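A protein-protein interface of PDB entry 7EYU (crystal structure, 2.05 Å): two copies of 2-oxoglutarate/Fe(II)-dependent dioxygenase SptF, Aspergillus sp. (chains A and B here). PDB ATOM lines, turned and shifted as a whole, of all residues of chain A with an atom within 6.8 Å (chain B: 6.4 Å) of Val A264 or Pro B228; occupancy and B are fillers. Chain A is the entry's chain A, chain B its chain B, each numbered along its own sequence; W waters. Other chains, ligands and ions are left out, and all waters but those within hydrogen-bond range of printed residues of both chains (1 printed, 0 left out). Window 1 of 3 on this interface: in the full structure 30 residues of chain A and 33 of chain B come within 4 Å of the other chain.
Trp A107 touches Thr B227, and with the chains exchanged Thr A227 touches Trp B107.
Thr B227 touches its own counterpart, Thr A227.
Positions printed for both chains: 107 and 227.
Of the 25 pairs that touch across the chains among the printed residues, 3 have their exchanged pair printed and touching as well.
Val A264 touches two residues of chain B.
Of chain A, only Val A264 and Trp A265 come within 4 Å of Pro B228.
Of the printed residues of chain B, His A225 touches Phe B131, Tyr B132, Phe B226 and Thr B227.
Printed residues of chain A within 4 Å of Phe B131: His A225 and Leu A258.
Of the printed residues of chain A, Ser B231 touches Trp A265 (3.2 Å) and Lys A266 (2.7 Å).
Printed residues of chain A within 4 Å of Ile B229: Val A262, Lys A263, Val A264, Trp A265 and Lys A266.
His B222 touches none of the printed residues of chain A.
Met B250 touches none of the printed residues of chain A.
The nearest residue of chain B that does not touch Val A264 is Thr B227 (4.3 Å).
The nearest residue of chain A that does not touch Pro B228 is Lys A266 (4.8 Å).
The nearest printed residue of chain B that does not touch Val A262 is Phe B131 (4.3 Å).
Among the printed residues, merely in contact across the chains: Trp A107 with Thr B227 (3.3 Å), His A225 with Phe B131 (3.6 Å), His A225 with Tyr B132 (3.3 Å), His A225 with Phe B226 (3.3 Å), Thr A227 with Trp B107 (3.2 Å), Thr A227 with Thr B227 (3.7 Å), Leu A258 with Phe B131 (3.2 Å), Asn A261 with Tyr B57 (3.5 Å), Val A262 with Tyr B57 (3.4 Å), Val A262 with Ile B229 (3.8 Å), Lys A263 with Ile B229 (3.3 Å), Val A264 with Pro B228 (3.8 Å), Val A264 with Ile B229 (3.6 Å), Trp A265 with Thr B227 (3.97 Å), Trp A265 with Ile B229 (3.6 Å), Trp A265 with Ser B231 (3.2 Å) and Lys A266 with Glu B230 (3.6 Å).
N of Trp B107 is in hydrogen-bond range of O of His B222, 3.0 Å away.
OH of Tyr B132 lies within hydrogen-bond range of ND2 of Asn B109 (2.8 Å).
The backbone carbonyl oxygen (O) of Asn B109 sits at hydrogen-bond distance from the backbone NH (N) of Ile B229, at 2.9 Å.
The backbone carbonyl oxygen (O) of Asp A105 sits at hydrogen-bond distance from the backbone NH (N) of Cys A224 (2.8 Å).
The side-chain hydroxyl of Thr A255 is in hydrogen-bond range of the backbone carbonyl oxygen of Trp A265, at 3.1 Å.
The backbone carbonyl oxygen of Leu A256 sits at hydrogen-bond distance from the backbone NH of Val A264 (3.0 Å).
OH of Tyr B57 lies within hydrogen-bond range of N of Lys A263 (2.9 Å).
OH of Tyr B57 is in hydrogen-bond range of NZ of Lys A266.
OG1 of Thr A227 is in hydrogen-bond range of O of Phe B226, at 3.0 Å.
OG1 of Thr B227 is in hydrogen-bond range of O of Cys A224, at 2.7 Å.
The backbone NH of Thr B227 lies within hydrogen-bond range of the backbone carbonyl oxygen of His A225 (2.7 Å).
The backbone NH (N) of Trp A265 sits at hydrogen-bond distance from the backbone carbonyl oxygen (O) of Pro B228 (2.9 Å).
The backbone NH (N) of Lys A266 sits at hydrogen-bond distance from the backbone carbonyl oxygen (O) of Ile B229 (3.1 Å).
The backbone carbonyl oxygen (O) of Lys A266 sits at hydrogen-bond distance from the backbone NH (N) of Ser B231 (2.7 Å).
Water W1 lies within hydrogen-bond range of OD1 of Asn B109 (2.7 Å), O of Thr B227 (2.7 Å), NE2 of His A225 (2.8 Å) and OH of Tyr B132 (3.2 Å).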
ATOM      1  N   ASP A 105      28.989  16.374   5.372  1.00  0.00           N
ATOM      2  CA  ASP A 105      28.246  15.995   4.187  1.00  0.00           C
ATOM      3  C   ASP A 105      28.845  16.655   2.951  1.00  0.00           C
ATOM      4  O   ASP A 105      29.561  17.658   3.031  1.00  0.00           O
ATOM      5  CB  ASP A 105      26.772  16.374   4.326  1.00  0.00           C
ATOM      6  CG  ASP A 105      25.960  15.321   5.065  1.00  0.00           C
ATOM      7  OD1 ASP A 105      26.541  14.305   5.503  1.00  0.00           O
ATOM      8  OD2 ASP A 105      24.728  15.492   5.174  1.00  0.00           O
ATOM      9  N   TRP A 107      27.934  17.058  -1.647  1.00  0.00           N
ATOM     10  CA  TRP A 107      26.907  16.926  -2.675  1.00  0.00           C
ATOM     11  C   TRP A 107      27.479  17.287  -4.040  1.00  0.00           C
ATOM     12  O   TRP A 107      28.619  17.742  -4.166  1.00  0.00           O
ATOM     13  CB  TRP A 107      25.661  17.768  -2.358  1.00  0.00           C
ATOM     14  CG  TRP A 107      25.880  19.239  -2.121  1.00  0.00           C
ATOM     15  CD1 TRP A 107      27.071  19.889  -1.963  1.00  0.00           C
ATOM     16  CD2 TRP A 107      24.860  20.240  -2.005  1.00  0.00           C
ATOM     17  NE1 TRP A 107      26.854  21.231  -1.761  1.00  0.00           N
ATOM     18  CE2 TRP A 107      25.504  21.472  -1.783  1.00  0.00           C
ATOM     19  CE3 TRP A 107      23.464  20.212  -2.073  1.00  0.00           C
ATOM     20  CZ2 TRP A 107      24.801  22.665  -1.625  1.00  0.00           C
ATOM     21  CZ3 TRP A 107      22.767  21.396  -1.916  1.00  0.00           C
ATOM     22  CH2 TRP A 107      23.436  22.607  -1.696  1.00  0.00           C
ATOM     23  N   CYS A 224      29.319  20.128   1.794  1.00  0.00           N
ATOM     24  CA  CYS A 224      27.927  20.551   1.905  1.00  0.00           C
ATOM     25  C   CYS A 224      27.789  22.065   1.941  1.00  0.00           C
ATOM     26  O   CYS A 224      26.800  22.605   1.430  1.00  0.00           O
ATOM     27  CB  CYS A 224      27.297  19.930   3.150  1.00  0.00           C
ATOM     28  SG  CYS A 224      28.214  20.285   4.658  1.00  0.00           S
ATOM     29  N   HIS A 225      28.754  22.761   2.537  1.00  0.00           N
ATOM     30  CA  HIS A 225      28.638  24.197   2.767  1.00  0.00           C
ATOM     31  C   HIS A 225      29.028  25.041   1.560  1.00  0.00           C
ATOM     32  O   HIS A 225      29.054  26.273   1.674  1.00  0.00           O
ATOM     33  CB  HIS A 225      29.494  24.616   3.971  1.00  0.00           C
ATOM     34  CG  HIS A 225      28.849  25.648   4.843  1.00  0.00           C
ATOM     35  ND1 HIS A 225      29.244  25.874   6.145  1.00  0.00           N
ATOM     36  CD2 HIS A 225      27.838  26.515   4.600  1.00  0.00           C
ATOM     37  CE1 HIS A 225      28.501  26.835   6.666  1.00  0.00           C
ATOM     38  NE2 HIS A 225      27.641  27.242   5.749  1.00  0.00           N
ATOM     39  N   THR A 227      28.381  26.183  -2.527  1.00  0.00           N
ATOM     40  CA  THR A 227      27.312  26.238  -3.520  1.00  0.00           C
ATOM     41  C   THR A 227      27.745  25.526  -4.797  1.00  0.00           C
ATOM     42  O   THR A 227      28.799  25.852  -5.353  1.00  0.00           O
ATOM     43  CB  THR A 227      26.939  27.685  -3.832  1.00  0.00           C
ATOM     44  OG1 THR A 227      26.554  28.351  -2.623  1.00  0.00           O
ATOM     45  CG2 THR A 227      25.783  27.736  -4.820  1.00  0.00           C
ATOM     46  N   ARG A 254      17.646  17.638  -0.610  1.00  0.00           N
ATOM     47  CA  ARG A 254      17.524  17.255   0.789  1.00  0.00           C
ATOM     48  C   ARG A 254      18.440  18.112   1.652  1.00  0.00           C
ATOM     49  O   ARG A 254      19.433  18.672   1.181  1.00  0.00           O
ATOM     50  CB  ARG A 254      17.853  15.768   0.994  1.00  0.00           C
ATOM     51  CG  ARG A 254      16.951  14.824   0.217  1.00  0.00           C
ATOM     52  CD  ARG A 254      16.850  13.467   0.892  1.00  0.00           C
ATOM     53  NE  ARG A 254      15.833  12.627   0.268  1.00  0.00           N
ATOM     54  CZ  ARG A 254      15.299  11.552   0.838  1.00  0.00           C
ATOM     55  NH1 ARG A 254      15.688  11.183   2.052  1.00  0.00           N
ATOM     56  NH2 ARG A 254      14.378  10.845   0.197  1.00  0.00           N
ATOM     57  N   THR A 255      18.089  18.202   2.933  1.00  0.00           N
ATOM     58  CA  THR A 255      18.905  18.925   3.898  1.00  0.00           C
ATOM     59  C   THR A 255      20.201  18.168   4.170  1.00  0.00           C
ATOM     60  O   THR A 255      20.211  16.936   4.267  1.00  0.00           O
ATOM     61  CB  THR A 255      18.119  19.126   5.198  1.00  0.00           C
ATOM     62  OG1 THR A 255      16.951  19.913   4.937  1.00  0.00           O
ATOM     63  CG2 THR A 255      18.964  19.816   6.253  1.00  0.00           C
ATOM     64  N   LEU A 256      21.298  18.911   4.283  1.00  0.00           N
ATOM     65  CA  LEU A 256      22.616  18.353   4.546  1.00  0.00           C
ATOM     66  C   LEU A 256      23.057  18.701   5.963  1.00  0.00           C
ATOM     67  O   LEU A 256      22.567  19.651   6.576  1.00  0.00           O
ATOM     68  CB  LEU A 256      23.644  18.863   3.532  1.00  0.00           C
ATOM     69  CG  LEU A 256      23.218  18.735   2.070  1.00  0.00           C
ATOM     70  CD1 LEU A 256      23.026  20.110   1.442  1.00  0.00           C
ATOM     71  CD2 LEU A 256      24.231  17.918   1.285  1.00  0.00           C
ATOM     72  N   ASN A 257      23.991  17.911   6.487  1.00  0.00           N
ATOM     73  CA  ASN A 257      24.426  18.019   7.875  1.00  0.00           C
ATOM     74  C   ASN A 257      25.898  18.413   7.929  1.00  0.00           C
ATOM     75  O   ASN A 257      26.734  17.765   7.292  1.00  0.00           O
ATOM     76  CB  ASN A 257      24.200  16.703   8.622  1.00  0.00           C
ATOM     77  CG  ASN A 257      22.750  16.269   8.612  1.00  0.00           C
ATOM     78  OD1 ASN A 257      21.933  16.776   9.381  1.00  0.00           O
ATOM     79  ND2 ASN A 257      22.420  15.331   7.736  1.00  0.00           N
ATOM     80  N   LEU A 258      26.219  19.466   8.690  1.00  0.00           N
ATOM     81  CA  LEU A 258      27.614  19.855   8.861  1.00  0.00           C
ATOM     82  C   LEU A 258      28.316  18.871   9.799  1.00  0.00           C
ATOM     83  O   LEU A 258      27.692  18.030  10.458  1.00  0.00           O
ATOM     84  CB  LEU A 258      27.744  21.298   9.371  1.00  0.00           C
ATOM     85  CG  LEU A 258      27.048  22.445   8.629  1.00  0.00           C
ATOM     86  CD1 LEU A 258      27.358  23.789   9.280  1.00  0.00           C
ATOM     87  CD2 LEU A 258      27.469  22.424   7.189  1.00  0.00           C
ATOM     88  N   ASN A 261      27.153  19.029  13.142  1.00  0.00           N
ATOM     89  CA  ASN A 261      25.764  18.577  13.176  1.00  0.00           C
ATOM     90  C   ASN A 261      24.759  19.690  12.912  1.00  0.00           C
ATOM     91  O   ASN A 261      23.550  19.436  12.972  1.00  0.00           O
ATOM     92  CB  ASN A 261      25.405  17.888  14.502  1.00  0.00           C
ATOM     93  CG  ASN A 261      26.254  16.662  14.767  1.00  0.00           C
ATOM     94  OD1 ASN A 261      26.134  15.649  14.077  1.00  0.00           O
ATOM     95  ND2 ASN A 261      27.119  16.746  15.772  1.00  0.00           N
ATOM     96  N   VAL A 262      25.205  20.913  12.630  1.00  0.00           N
ATOM     97  CA  VAL A 262      24.288  21.957  12.193  1.00  0.00           C
ATOM     98  C   VAL A 262      23.830  21.637  10.778  1.00  0.00           C
ATOM     99  O   VAL A 262      24.626  21.204   9.937  1.00  0.00           O
ATOM    100  CB  VAL A 262      24.963  23.335  12.280  1.00  0.00           C
ATOM    101  CG1 VAL A 262      24.087  24.412  11.657  1.00  0.00           C
ATOM    102  CG2 VAL A 262      25.288  23.675  13.729  1.00  0.00           C
ATOM    103  N   LYS A 263      22.541  21.810  10.512  1.00  0.00           N
ATOM    104  CA  LYS A 263      21.996  21.476   9.205  1.00  0.00           C
ATOM    105  C   LYS A 263      21.973  22.710   8.311  1.00  0.00           C
ATOM    106  O   LYS A 263      21.487  23.771   8.715  1.00  0.00           O
ATOM    107  CB  LYS A 263      20.588  20.894   9.332  1.00  0.00           C
ATOM    108  CG  LYS A 263      20.490  19.621  10.149  1.00  0.00           C
ATOM    109  CD  LYS A 263      19.095  19.027  10.033  1.00  0.00           C
ATOM    110  CE  LYS A 263      18.758  18.151  11.225  1.00  0.00           C
ATOM    111  NZ  LYS A 263      17.322  17.756  11.221  1.00  0.00           N
ATOM    112  N   VAL A 264      22.511  22.569   7.102  1.00  0.00           N
ATOM    113  CA  VAL A 264      22.408  23.597   6.080  1.00  0.00           C
ATOM    114  C   VAL A 264      21.371  23.157   5.059  1.00  0.00           C
ATOM    115  O   VAL A 264      20.938  22.001   5.027  1.00  0.00           O
ATOM    116  CB  VAL A 264      23.753  23.895   5.381  1.00  0.00           C
ATOM    117  CG1 VAL A 264      24.726  24.547   6.337  1.00  0.00           C
ATOM    118  CG2 VAL A 264      24.335  22.621   4.792  1.00  0.00           C
ATOM    119  N   TRP A 265      20.980  24.096   4.198  1.00  0.00           N
ATOM    120  CA  TRP A 265      19.975  23.839   3.171  1.00  0.00           C
ATOM    121  C   TRP A 265      18.688  23.308   3.800  1.00  0.00           C
ATOM    122  O   TRP A 265      18.115  22.313   3.353  1.00  0.00           O
ATOM    123  CB  TRP A 265      20.517  22.876   2.110  1.00  0.00           C
ATOM    124  CG  TRP A 265      19.859  23.012   0.782  1.00  0.00           C
ATOM    125  CD1 TRP A 265      19.187  22.042   0.098  1.00  0.00           C
ATOM    126  CD2 TRP A 265      19.810  24.187  -0.033  1.00  0.00           C
ATOM    127  NE1 TRP A 265      18.721  22.541  -1.093  1.00  0.00           N
ATOM    128  CE2 TRP A 265      19.090  23.856  -1.197  1.00  0.00           C
ATOM    129  CE3 TRP A 265      20.304  25.487   0.110  1.00  0.00           C
ATOM    130  CZ2 TRP A 265      18.851  24.779  -2.213  1.00  0.00           C
ATOM    131  CZ3 TRP A 265      20.068  26.398  -0.899  1.00  0.00           C
ATOM    132  CH2 TRP A 265      19.348  26.043  -2.045  1.00  0.00           C
ATOM    133  N   LYS A 266      18.238  23.979   4.858  1.00  0.00           N
ATOM    134  CA  LYS A 266      17.102  23.510   5.636  1.00  0.00           C
ATOM    135  C   LYS A 266      15.780  24.071   5.105  1.00  0.00           C
ATOM    136  O   LYS A 266      15.741  24.993   4.286  1.00  0.00           O
ATOM    137  CB  LYS A 266      17.263  23.878   7.110  1.00  0.00           C
ATOM    138  CG  LYS A 266      18.129  22.935   7.898  1.00  0.00           C
ATOM    139  CD  LYS A 266      17.830  23.110   9.369  1.00  0.00           C
ATOM    140  CE  LYS A 266      18.165  24.522   9.808  1.00  0.00           C
ATOM    141  NZ  LYS A 266      19.619  24.801   9.662  1.00  0.00           N
ATOM    142  N   ALA A 267      14.687  23.454   5.560  1.00  0.00           N
ATOM    143  CA  ALA A 267      13.326  23.942   5.335  1.00  0.00           C
ATOM    144  C   ALA A 267      12.900  24.622   6.630  1.00  0.00           C
ATOM    145  O   ALA A 267      12.214  24.038   7.472  1.00  0.00           O
ATOM    146  CB  ALA A 267      12.379  22.810   4.962  1.00  0.00           C
ATOM    147  N   TYR B  57      16.443  20.799  16.363  1.00  0.00           N
ATOM    148  CA  TYR B  57      17.268  19.623  16.136  1.00  0.00           C
ATOM    149  C   TYR B  57      18.559  19.753  16.934  1.00  0.00           C
ATOM    150  O   TYR B  57      18.951  20.847  17.349  1.00  0.00           O
ATOM    151  CB  TYR B  57      17.574  19.419  14.643  1.00  0.00           C
ATOM    152  CG  TYR B  57      18.450  20.487  14.027  1.00  0.00           C
ATOM    153  CD1 TYR B  57      17.906  21.680  13.572  1.00  0.00           C
ATOM    154  CD2 TYR B  57      19.819  20.295  13.891  1.00  0.00           C
ATOM    155  CE1 TYR B  57      18.703  22.657  13.003  1.00  0.00           C
ATOM    156  CE2 TYR B  57      20.623  21.266  13.326  1.00  0.00           C
ATOM    157  CZ  TYR B  57      20.060  22.444  12.883  1.00  0.00           C
ATOM    158  OH  TYR B  57      20.859  23.412  12.319  1.00  0.00           O
ATOM    159  N   TRP B 107      23.994  36.194  -1.234  1.00  0.00           N
ATOM    160  CA  TRP B 107      22.581  35.843  -1.180  1.00  0.00           C
ATOM    161  C   TRP B 107      22.185  35.565   0.265  1.00  0.00           C
ATOM    162  O   TRP B 107      23.007  35.625   1.183  1.00  0.00           O
ATOM    163  CB  TRP B 107      22.249  34.660  -2.099  1.00  0.00           C
ATOM    164  CG  TRP B 107      23.036  33.396  -1.879  1.00  0.00           C
ATOM    165  CD1 TRP B 107      24.145  33.230  -1.099  1.00  0.00           C
ATOM    166  CD2 TRP B 107      22.767  32.119  -2.468  1.00  0.00           C
ATOM    167  NE1 TRP B 107      24.579  31.928  -1.164  1.00  0.00           N
ATOM    168  CE2 TRP B 107      23.749  31.225  -1.998  1.00  0.00           C
ATOM    169  CE3 TRP B 107      21.787  31.645  -3.346  1.00  0.00           C
ATOM    170  CZ2 TRP B 107      23.780  29.886  -2.379  1.00  0.00           C
ATOM    171  CZ3 TRP B 107      21.821  30.316  -3.723  1.00  0.00           C
ATOM    172  CH2 TRP B 107      22.809  29.451  -3.238  1.00  0.00           C
ATOM    173  N   PHE B 108      20.903  35.264   0.449  1.00  0.00           N
ATOM    174  CA  PHE B 108      20.328  35.092   1.774  1.00  0.00           C
ATOM    175  C   PHE B 108      20.866  33.829   2.434  1.00  0.00           C
ATOM    176  O   PHE B 108      20.781  32.734   1.868  1.00  0.00           O
ATOM    177  CB  PHE B 108      18.806  35.032   1.660  1.00  0.00           C
ATOM    178  CG  PHE B 108      18.088  35.057   2.975  1.00  0.00           C
ATOM    179  CD1 PHE B 108      18.114  36.187   3.776  1.00  0.00           C
ATOM    180  CD2 PHE B 108      17.359  33.960   3.396  1.00  0.00           C
ATOM    181  CE1 PHE B 108      17.441  36.212   4.980  1.00  0.00           C
ATOM    182  CE2 PHE B 108      16.682  33.979   4.598  1.00  0.00           C
ATOM    183  CZ  PHE B 108      16.721  35.108   5.390  1.00  0.00           C
ATOM    184  N   ASN B 109      21.421  33.982   3.637  1.00  0.00           N
ATOM    185  CA  ASN B 109      21.934  32.851   4.398  1.00  0.00           C
ATOM    186  C   ASN B 109      20.859  32.243   5.295  1.00  0.00           C
ATOM    187  O   ASN B 109      20.620  31.032   5.251  1.00  0.00           O
ATOM    188  CB  ASN B 109      23.143  33.285   5.233  1.00  0.00           C
ATOM    189  CG  ASN B 109      23.887  32.111   5.844  1.00  0.00           C
ATOM    190  OD1 ASN B 109      23.617  30.954   5.523  1.00  0.00           O
ATOM    191  ND2 ASN B 109      24.834  32.406   6.726  1.00  0.00           N
ATOM    192  N   GLY B 110      20.205  33.067   6.102  1.00  0.00           N
ATOM    193  CA  GLY B 110      19.159  32.581   6.982  1.00  0.00           C
ATOM    194  C   GLY B 110      18.539  33.738   7.735  1.00  0.00           C
ATOM    195  O   GLY B 110      19.078  34.848   7.772  1.00  0.00           O
ATOM    196  N   PHE B 131      29.754  28.063  12.964  1.00  0.00           N
ATOM    197  CA  PHE B 131      29.341  26.866  12.241  1.00  0.00           C
ATOM    198  C   PHE B 131      29.951  26.775  10.850  1.00  0.00           C
ATOM    199  O   PHE B 131      29.641  25.832  10.114  1.00  0.00           O
ATOM    200  CB  PHE B 131      27.811  26.791  12.161  1.00  0.00           C
ATOM    201  CG  PHE B 131      27.190  27.789  11.226  1.00  0.00           C
ATOM    202  CD1 PHE B 131      26.964  29.093  11.633  1.00  0.00           C
ATOM    203  CD2 PHE B 131      26.807  27.416   9.947  1.00  0.00           C
ATOM    204  CE1 PHE B 131      26.382  30.010  10.778  1.00  0.00           C
ATOM    205  CE2 PHE B 131      26.228  28.329   9.087  1.00  0.00           C
ATOM    206  CZ  PHE B 131      26.011  29.627   9.504  1.00  0.00           C
ATOM    207  N   TYR B 132      30.806  27.720  10.471  1.00  0.00           N
ATOM    208  CA  TYR B 132      31.603  27.607   9.256  1.00  0.00           C
ATOM    209  C   TYR B 132      32.906  26.895   9.598  1.00  0.00           C
ATOM    210  O   TYR B 132      33.658  27.354  10.464  1.00  0.00           O
ATOM    211  CB  TYR B 132      31.888  28.983   8.654  1.00  0.00           C
ATOM    212  CG  TYR B 132      30.696  29.641   8.000  1.00  0.00           C
ATOM    213  CD1 TYR B 132      29.811  30.412   8.742  1.00  0.00           C
ATOM    214  CD2 TYR B 132      30.460  29.502   6.638  1.00  0.00           C
ATOM    215  CE1 TYR B 132      28.724  31.021   8.147  1.00  0.00           C
ATOM    216  CE2 TYR B 132      29.373  30.105   6.036  1.00  0.00           C
ATOM    217  CZ  TYR B 132      28.507  30.862   6.796  1.00  0.00           C
ATOM    218  OH  TYR B 132      27.422  31.468   6.206  1.00  0.00           O
ATOM    219  N   HIS B 222      25.407  35.965   3.047  1.00  0.00           N
ATOM    220  CA  HIS B 222      26.757  35.428   2.958  1.00  0.00           C
ATOM    221  C   HIS B 222      27.111  35.254   1.483  1.00  0.00           C
ATOM    222  O   HIS B 222      26.231  35.315   0.622  1.00  0.00           O
ATOM    223  CB  HIS B 222      26.881  34.103   3.727  1.00  0.00           C
ATOM    224  CG  HIS B 222      26.106  32.971   3.132  1.00  0.00           C
ATOM    225  ND1 HIS B 222      26.326  31.657   3.485  1.00  0.00           N
ATOM    226  CD2 HIS B 222      25.110  32.952   2.214  1.00  0.00           C
ATOM    227  CE1 HIS B 222      25.504  30.878   2.806  1.00  0.00           C
ATOM    228  NE2 HIS B 222      24.756  31.637   2.027  1.00  0.00           N
ATOM    229  N   PHE B 226      28.714  30.033  -0.771  1.00  0.00           N
ATOM    230  CA  PHE B 226      28.440  29.322   0.469  1.00  0.00           C
ATOM    231  C   PHE B 226      26.990  28.852   0.488  1.00  0.00           C
ATOM    232  O   PHE B 226      26.086  29.578   0.062  1.00  0.00           O
ATOM    233  CB  PHE B 226      28.719  30.205   1.691  1.00  0.00           C
ATOM    234  CG  PHE B 226      30.146  30.670   1.793  1.00  0.00           C
ATOM    235  CD1 PHE B 226      31.165  29.972   1.166  1.00  0.00           C
ATOM    236  CD2 PHE B 226      30.467  31.804   2.520  1.00  0.00           C
ATOM    237  CE1 PHE B 226      32.476  30.397   1.259  1.00  0.00           C
ATOM    238  CE2 PHE B 226      31.777  32.235   2.617  1.00  0.00           C
ATOM    239  CZ  PHE B 226      32.783  31.529   1.985  1.00  0.00           C
ATOM    240  N   THR B 227      26.775  27.637   0.978  1.00  0.00           N
ATOM    241  CA  THR B 227      25.426  27.086   1.032  1.00  0.00           C
ATOM    242  C   THR B 227      24.638  27.755   2.154  1.00  0.00           C
ATOM    243  O   THR B 227      25.113  27.801   3.296  1.00  0.00           O
ATOM    244  CB  THR B 227      25.472  25.576   1.249  1.00  0.00           C
ATOM    245  OG1 THR B 227      26.225  24.963   0.193  1.00  0.00           O
ATOM    246  CG2 THR B 227      24.066  24.993   1.266  1.00  0.00           C
ATOM    247  N   PRO B 228      23.450  28.284   1.878  1.00  0.00           N
ATOM    248  CA  PRO B 228      22.675  28.938   2.936  1.00  0.00           C
ATOM    249  C   PRO B 228      22.153  27.935   3.950  1.00  0.00           C
ATOM    250  O   PRO B 228      21.922  26.763   3.643  1.00  0.00           O
ATOM    251  CB  PRO B 228      21.521  29.608   2.176  1.00  0.00           C
ATOM    252  CG  PRO B 228      21.940  29.607   0.734  1.00  0.00           C
ATOM    253  CD  PRO B 228      22.788  28.389   0.568  1.00  0.00           C
ATOM    254  N   ILE B 229      21.970  28.417   5.182  1.00  0.00           N
ATOM    255  CA  ILE B 229      21.393  27.581   6.226  1.00  0.00           C
ATOM    256  C   ILE B 229      19.932  27.269   5.940  1.00  0.00           C
ATOM    257  O   ILE B 229      19.386  26.308   6.494  1.00  0.00           O
ATOM    258  CB  ILE B 229      21.552  28.258   7.602  1.00  0.00           C
ATOM    259  CG1 ILE B 229      21.710  27.206   8.702  1.00  0.00           C
ATOM    260  CG2 ILE B 229      20.371  29.171   7.903  1.00  0.00           C
ATOM    261  CD1 ILE B 229      23.097  26.621   8.790  1.00  0.00           C
ATOM    262  N   GLU B 230      19.287  28.046   5.073  1.00  0.00           N
ATOM    263  CA  GLU B 230      17.879  27.874   4.748  1.00  0.00           C
ATOM    264  C   GLU B 230      17.709  27.844   3.239  1.00  0.00           C
ATOM    265  O   GLU B 230      18.190  28.740   2.539  1.00  0.00           O
ATOM    266  CB  GLU B 230      17.030  29.005   5.341  1.00  0.00           C
ATOM    267  CG  GLU B 230      16.631  28.808   6.790  1.00  0.00           C
ATOM    268  CD  GLU B 230      15.898  30.012   7.351  1.00  0.00           C
ATOM    269  OE1 GLU B 230      14.701  30.182   7.035  1.00  0.00           O
ATOM    270  OE2 GLU B 230      16.519  30.789   8.106  1.00  0.00           O
ATOM    271  N   SER B 231      17.033  26.814   2.744  1.00  0.00           N
ATOM    272  CA  SER B 231      16.586  26.778   1.363  1.00  0.00           C
ATOM    273  C   SER B 231      15.165  27.326   1.274  1.00  0.00           C
ATOM    274  O   SER B 231      14.435  27.385   2.265  1.00  0.00           O
ATOM    275  CB  SER B 231      16.644  25.354   0.806  1.00  0.00           C
ATOM    276  OG  SER B 231      16.183  25.308  -0.534  1.00  0.00           O
ATOM    277  N   HIS B 232      14.779  27.736   0.065  1.00  0.00           N
ATOM    278  CA  HIS B 232      13.474  28.350  -0.138  1.00  0.00           C
ATOM    279  C   HIS B 232      12.707  27.759  -1.315  1.00  0.00           C
ATOM    280  O   HIS B 232      11.706  28.346  -1.740  1.00  0.00           O
ATOM    281  CB  HIS B 232      13.623  29.866  -0.318  1.00  0.00           C
ATOM    282  CG  HIS B 232      14.085  30.573   0.918  1.00  0.00           C
ATOM    283  ND1 HIS B 232      15.414  30.672   1.267  1.00  0.00           N
ATOM    284  CD2 HIS B 232      13.392  31.207   1.894  1.00  0.00           C
ATOM    285  CE1 HIS B 232      15.522  31.339   2.402  1.00  0.00           C
ATOM    286  NE2 HIS B 232      14.309  31.676   2.803  1.00  0.00           N
ATOM    287  N   MET B 250      18.145  36.525  -4.064  1.00  0.00           N
ATOM    288  CA  MET B 250      18.538  36.335  -2.672  1.00  0.00           C
ATOM    289  C   MET B 250      18.153  34.949  -2.174  1.00  0.00           C
ATOM    290  O   MET B 250      18.916  34.310  -1.439  1.00  0.00           O
ATOM    291  CB  MET B 250      17.894  37.408  -1.793  1.00  0.00           C
ATOM    292  CG  MET B 250      18.528  38.788  -1.888  1.00  0.00           C
ATOM    293  SD  MET B 250      20.285  38.815  -1.493  1.00  0.00           S
ATOM    294  CE  MET B 250      20.996  39.083  -3.113  1.00  0.00           C
HETATM  295  O   HOH W   1      25.415  28.993   5.703  1.00  0.00           O
